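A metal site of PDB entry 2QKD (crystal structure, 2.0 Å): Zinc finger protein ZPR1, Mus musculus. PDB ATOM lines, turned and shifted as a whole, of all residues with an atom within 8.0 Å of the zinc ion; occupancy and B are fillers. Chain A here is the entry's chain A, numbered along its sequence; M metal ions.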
ATOM      1  N   SER A  13     -14.695   8.119  20.727  1.00  0.00           N
ATOM      2  CA  SER A  13     -14.866   7.697  22.107  1.00  0.00           C
ATOM      3  C   SER A  13     -14.290   8.758  23.018  1.00  0.00           C
ATOM      4  O   SER A  13     -13.308   9.409  22.688  1.00  0.00           O
ATOM      5  CB  SER A  13     -14.128   6.379  22.354  1.00  0.00           C
ATOM      6  OG  SER A  13     -14.317   5.494  21.273  1.00  0.00           O
ATOM      7  N   LEU A  14     -14.902   8.915  24.191  1.00  0.00           N
ATOM      8  CA  LEU A  14     -14.446   9.872  25.189  1.00  0.00           C
ATOM      9  C   LEU A  14     -13.052   9.520  25.713  1.00  0.00           C
ATOM     10  O   LEU A  14     -12.798   8.353  26.040  1.00  0.00           O
ATOM     11  CB  LEU A  14     -15.449   9.924  26.334  1.00  0.00           C
ATOM     12  CG  LEU A  14     -15.391  11.060  27.348  1.00  0.00           C
ATOM     13  CD1 LEU A  14     -15.746  12.373  26.688  1.00  0.00           C
ATOM     14  CD2 LEU A  14     -16.343  10.773  28.486  1.00  0.00           C
ATOM     15  N   CYS A  15     -12.145  10.491  25.750  1.00  0.00           N
ATOM     16  CA  CYS A  15     -10.841  10.320  26.400  1.00  0.00           C
ATOM     17  C   CYS A  15     -10.973  10.457  27.913  1.00  0.00           C
ATOM     18  O   CYS A  15     -11.451  11.475  28.404  1.00  0.00           O
ATOM     19  CB  CYS A  15      -9.840  11.348  25.878  1.00  0.00           C
ATOM     20  SG  CYS A  15      -8.201  11.182  26.603  1.00  0.00           S
ATOM     21  N   MET A  16     -10.521   9.446  28.660  1.00  0.00           N
ATOM     22  CA  MET A  16     -10.638   9.506  30.107  1.00  0.00           C
ATOM     23  C   MET A  16      -9.570  10.401  30.740  1.00  0.00           C
ATOM     24  O   MET A  16      -9.664  10.726  31.922  1.00  0.00           O
ATOM     25  CB  MET A  16     -10.595   8.102  30.746  1.00  0.00           C
ATOM     26  CG  MET A  16     -11.787   7.184  30.444  1.00  0.00           C
ATOM     27  SD  MET A  16     -13.384   7.743  31.059  1.00  0.00           S
ATOM     28  CE  MET A  16     -14.126   8.239  29.526  1.00  0.00           C
ATOM     29  N   ASN A  17      -8.561  10.786  29.964  1.00  0.00           N
ATOM     30  CA  ASN A  17      -7.458  11.613  30.450  1.00  0.00           C
ATOM     31  C   ASN A  17      -7.690  13.119  30.293  1.00  0.00           C
ATOM     32  O   ASN A  17      -7.110  13.914  31.016  1.00  0.00           O
ATOM     33  CB  ASN A  17      -6.148  11.205  29.768  1.00  0.00           C
ATOM     34  CG  ASN A  17      -4.922  11.851  30.392  1.00  0.00           C
ATOM     35  OD1 ASN A  17      -4.175  12.568  29.723  1.00  0.00           O
ATOM     36  ND2 ASN A  17      -4.706  11.594  31.670  1.00  0.00           N
ATOM     37  N   CYS A  18      -8.555  13.520  29.359  1.00  0.00           N
ATOM     38  CA  CYS A  18      -8.759  14.956  29.084  1.00  0.00           C
ATOM     39  C   CYS A  18     -10.212  15.319  28.738  1.00  0.00           C
ATOM     40  O   CYS A  18     -10.560  16.508  28.667  1.00  0.00           O
ATOM     41  CB  CYS A  18      -7.819  15.438  27.980  1.00  0.00           C
ATOM     42  SG  CYS A  18      -8.374  15.102  26.265  1.00  0.00           S
ATOM     43  N   TYR A  19     -11.034  14.301  28.528  1.00  0.00           N
ATOM     44  CA  TYR A  19     -12.483  14.432  28.242  1.00  0.00           C
ATOM     45  C   TYR A  19     -12.846  15.098  26.912  1.00  0.00           C
ATOM     46  O   TYR A  19     -13.988  15.504  26.719  1.00  0.00           O
ATOM     47  CB  TYR A  19     -13.276  14.993  29.428  1.00  0.00           C
ATOM     48  CG  TYR A  19     -13.946  13.935  30.301  1.00  0.00           C
ATOM     49  CD1 TYR A  19     -13.248  12.793  30.701  1.00  0.00           C
ATOM     50  CD2 TYR A  19     -15.267  14.089  30.727  1.00  0.00           C
ATOM     51  CE1 TYR A  19     -13.857  11.817  31.500  1.00  0.00           C
ATOM     52  CE2 TYR A  19     -15.883  13.109  31.531  1.00  0.00           C
ATOM     53  CZ  TYR A  19     -15.163  11.974  31.909  1.00  0.00           C
ATOM     54  OH  TYR A  19     -15.751  10.992  32.712  1.00  0.00           O
ATOM     55  N   ARG A  20     -11.886  15.158  25.998  1.00  0.00           N
ATOM     56  CA  ARG A  20     -12.181  15.347  24.585  1.00  0.00           C
ATOM     57  C   ARG A  20     -12.603  14.002  23.982  1.00  0.00           C
ATOM     58  O   ARG A  20     -12.634  12.993  24.702  1.00  0.00           O
ATOM     59  CB  ARG A  20     -10.956  15.927  23.878  1.00  0.00           C
ATOM     60  CG  ARG A  20     -10.707  17.380  24.248  1.00  0.00           C
ATOM     61  CD  ARG A  20      -9.348  17.893  23.793  1.00  0.00           C
ATOM     62  NE  ARG A  20      -9.049  19.216  24.357  1.00  0.00           N
ATOM     63  CZ  ARG A  20      -8.479  19.425  25.534  1.00  0.00           C
ATOM     64  NH1 ARG A  20      -8.134  18.397  26.308  1.00  0.00           N
ATOM     65  NH2 ARG A  20      -8.238  20.676  25.952  1.00  0.00           N
ATOM     66  N   ASN A  21     -12.947  13.986  22.691  1.00  0.00           N
ATOM     67  CA  ASN A  21     -13.194  12.738  21.975  1.00  0.00           C
ATOM     68  C   ASN A  21     -11.921  12.313  21.244  1.00  0.00           C
ATOM     69  O   ASN A  21     -11.326  13.102  20.518  1.00  0.00           O
ATOM     70  CB  ASN A  21     -14.350  12.885  20.969  1.00  0.00           C
ATOM     71  CG  ASN A  21     -15.724  12.938  21.641  1.00  0.00           C
ATOM     72  OD1 ASN A  21     -15.888  12.566  22.801  1.00  0.00           O
ATOM     73  ND2 ASN A  21     -16.724  13.385  20.886  1.00  0.00           N
ATOM     74  N   GLY A  22     -11.505  11.068  21.463  1.00  0.00           N
ATOM     75  CA  GLY A  22     -10.402  10.466  20.726  1.00  0.00           C
ATOM     76  C   GLY A  22     -10.929   9.401  19.785  1.00  0.00           C
ATOM     77  O   GLY A  22     -12.127   9.400  19.451  1.00  0.00           O
ATOM     78  N   PHE A  42      -7.616   2.479  22.103  1.00  0.00           N
ATOM     79  CA  PHE A  42      -7.941   3.914  22.180  1.00  0.00           C
ATOM     80  C   PHE A  42      -6.716   4.811  22.062  1.00  0.00           C
ATOM     81  O   PHE A  42      -5.644   4.516  22.603  1.00  0.00           O
ATOM     82  CB  PHE A  42      -8.714   4.243  23.467  1.00  0.00           C
ATOM     83  CG  PHE A  42      -8.991   5.725  23.634  1.00  0.00           C
ATOM     84  CD1 PHE A  42     -10.149   6.290  23.088  1.00  0.00           C
ATOM     85  CD2 PHE A  42      -8.098   6.553  24.308  1.00  0.00           C
ATOM     86  CE1 PHE A  42     -10.386   7.656  23.211  1.00  0.00           C
ATOM     87  CE2 PHE A  42      -8.327   7.930  24.433  1.00  0.00           C
ATOM     88  CZ  PHE A  42      -9.473   8.467  23.900  1.00  0.00           C
ATOM     89  N   SER A  43      -6.875   5.928  21.338  1.00  0.00           N
ATOM     90  CA  SER A  43      -5.849   6.975  21.359  1.00  0.00           C
ATOM     91  C   SER A  43      -6.441   8.394  21.253  1.00  0.00           C
ATOM     92  O   SER A  43      -7.465   8.606  20.591  1.00  0.00           O
ATOM     93  CB  SER A  43      -4.808   6.754  20.278  1.00  0.00           C
ATOM     94  OG  SER A  43      -5.407   6.836  19.000  1.00  0.00           O
ATOM     95  N   CYS A  44      -5.794   9.333  21.924  1.00  0.00           N
ATOM     96  CA  CYS A  44      -6.187  10.748  21.887  1.00  0.00           C
ATOM     97  C   CYS A  44      -5.026  11.572  21.340  1.00  0.00           C
ATOM     98  O   CYS A  44      -3.975  11.694  21.978  1.00  0.00           O
ATOM     99  CB  CYS A  44      -6.578  11.226  23.285  1.00  0.00           C
ATOM    100  SG  CYS A  44      -7.104  12.984  23.373  1.00  0.00           S
ATOM    101  N   GLU A  45      -5.215  12.144  20.157  1.00  0.00           N
ATOM    102  CA  GLU A  45      -4.208  12.998  19.552  1.00  0.00           C
ATOM    103  C   GLU A  45      -3.950  14.280  20.374  1.00  0.00           C
ATOM    104  O   GLU A  45      -2.851  14.831  20.301  1.00  0.00           O
ATOM    105  CB  GLU A  45      -4.602  13.373  18.119  1.00  0.00           C
ATOM    106  CG  GLU A  45      -5.149  12.222  17.252  1.00  0.00           C
ATOM    107  CD  GLU A  45      -4.187  11.050  17.106  1.00  0.00           C
ATOM    108  OE1 GLU A  45      -2.995  11.303  16.811  1.00  0.00           O
ATOM    109  OE2 GLU A  45      -4.637   9.887  17.286  1.00  0.00           O
ATOM    110  N   HIS A  46      -4.935  14.743  21.139  1.00  0.00           N
ATOM    111  CA  HIS A  46      -4.799  16.031  21.868  1.00  0.00           C
ATOM    112  C   HIS A  46      -3.890  15.934  23.090  1.00  0.00           C
ATOM    113  O   HIS A  46      -2.940  16.708  23.233  1.00  0.00           O
ATOM    114  CB  HIS A  46      -6.150  16.615  22.253  1.00  0.00           C
ATOM    115  CG  HIS A  46      -6.135  18.105  22.496  1.00  0.00           C
ATOM    116  ND1 HIS A  46      -5.679  18.664  23.676  1.00  0.00           N
ATOM    117  CD2 HIS A  46      -6.515  19.134  21.711  1.00  0.00           C
ATOM    118  CE1 HIS A  46      -5.782  19.979  23.597  1.00  0.00           C
ATOM    119  NE2 HIS A  46      -6.283  20.295  22.429  1.00  0.00           N
ATOM    120  N   CYS A  47      -4.190  14.986  23.986  1.00  0.00           N
ATOM    121  CA  CYS A  47      -3.407  14.812  25.212  1.00  0.00           C
ATOM    122  C   CYS A  47      -2.422  13.652  25.151  1.00  0.00           C
ATOM    123  O   CYS A  47      -1.625  13.457  26.086  1.00  0.00           O
ATOM    124  CB  CYS A  47      -4.335  14.642  26.429  1.00  0.00           C
ATOM    125  SG  CYS A  47      -5.108  12.987  26.577  1.00  0.00           S
ATOM    126  N   GLY A  48      -2.475  12.863  24.075  1.00  0.00           N
ATOM    127  CA  GLY A  48      -1.501  11.770  23.879  1.00  0.00           C
ATOM    128  C   GLY A  48      -1.809  10.477  24.639  1.00  0.00           C
ATOM    129  O   GLY A  48      -1.067   9.477  24.542  1.00  0.00           O
ATOM    130  N   TRP A  49      -2.902  10.477  25.394  1.00  0.00           N
ATOM    131  CA  TRP A  49      -3.264   9.297  26.174  1.00  0.00           C
ATOM    132  C   TRP A  49      -3.642   8.139  25.269  1.00  0.00           C
ATOM    133  O   TRP A  49      -4.130   8.329  24.126  1.00  0.00           O
ATOM    134  CB  TRP A  49      -4.388   9.580  27.131  1.00  0.00           C
ATOM    135  CG  TRP A  49      -4.536   8.532  28.197  1.00  0.00           C
ATOM    136  CD1 TRP A  49      -3.627   8.221  29.193  1.00  0.00           C
ATOM    137  CD2 TRP A  49      -5.650   7.665  28.401  1.00  0.00           C
ATOM    138  NE1 TRP A  49      -4.117   7.217  29.980  1.00  0.00           N
ATOM    139  CE2 TRP A  49      -5.353   6.856  29.513  1.00  0.00           C
ATOM    140  CE3 TRP A  49      -6.867   7.498  27.739  1.00  0.00           C
ATOM    141  CZ2 TRP A  49      -6.251   5.884  29.997  1.00  0.00           C
ATOM    142  CZ3 TRP A  49      -7.751   6.528  28.206  1.00  0.00           C
ATOM    143  CH2 TRP A  49      -7.431   5.737  29.326  1.00  0.00           C
ATOM    144  N   ASN A  50      -3.386   6.942  25.767  1.00  0.00           N
ATOM    145  CA  ASN A  50      -3.667   5.725  25.010  1.00  0.00           C
ATOM    146  C   ASN A  50      -3.923   4.587  25.978  1.00  0.00           C
ATOM    147  O   ASN A  50      -3.367   4.542  27.070  1.00  0.00           O
ATOM    148  CB  ASN A  50      -2.504   5.395  24.068  1.00  0.00           C
ATOM    149  CG  ASN A  50      -1.149   5.406  24.773  1.00  0.00           C
ATOM    150  OD1 ASN A  50      -0.563   6.476  25.039  1.00  0.00           O
ATOM    151  ND2 ASN A  50      -0.628   4.213  25.071  1.00  0.00           N
HETATM  152 ZN    ZN M   1      -7.208  13.096  25.726  1.00  0.00          ZN
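SG of Cys 47 sits close to OD1 of Asn 17 (3.3 Å). The side-chain sulfur (SG) of Cys 47 lies close to the backbone NH (N) of Trp 49 (3.5 Å). N of Asn 17 sits close to SG of Cys 15, 3.4 Å away. N of Cys 15 is in hydrogen-bond range of O of Arg 20 (2.8 Å). N of Cys 44 sits at hydrogen-bond distance from O of Trp 49, at 2.9 Å. The side-chain sulfur (SG) of Cys 44 sits close to the backbone NH (N) of His 46, at 3.6 Å. The side-chain sulfur of Cys 18 lies close to the guanidinium group of Arg 20.
The zinc ion is bound by SG of Cys 47, SG of Cys 15, SG of Cys 44 and SG of Cys 18.
Of the 19 residues printed, 4 come within 4 Å of the zinc ion.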
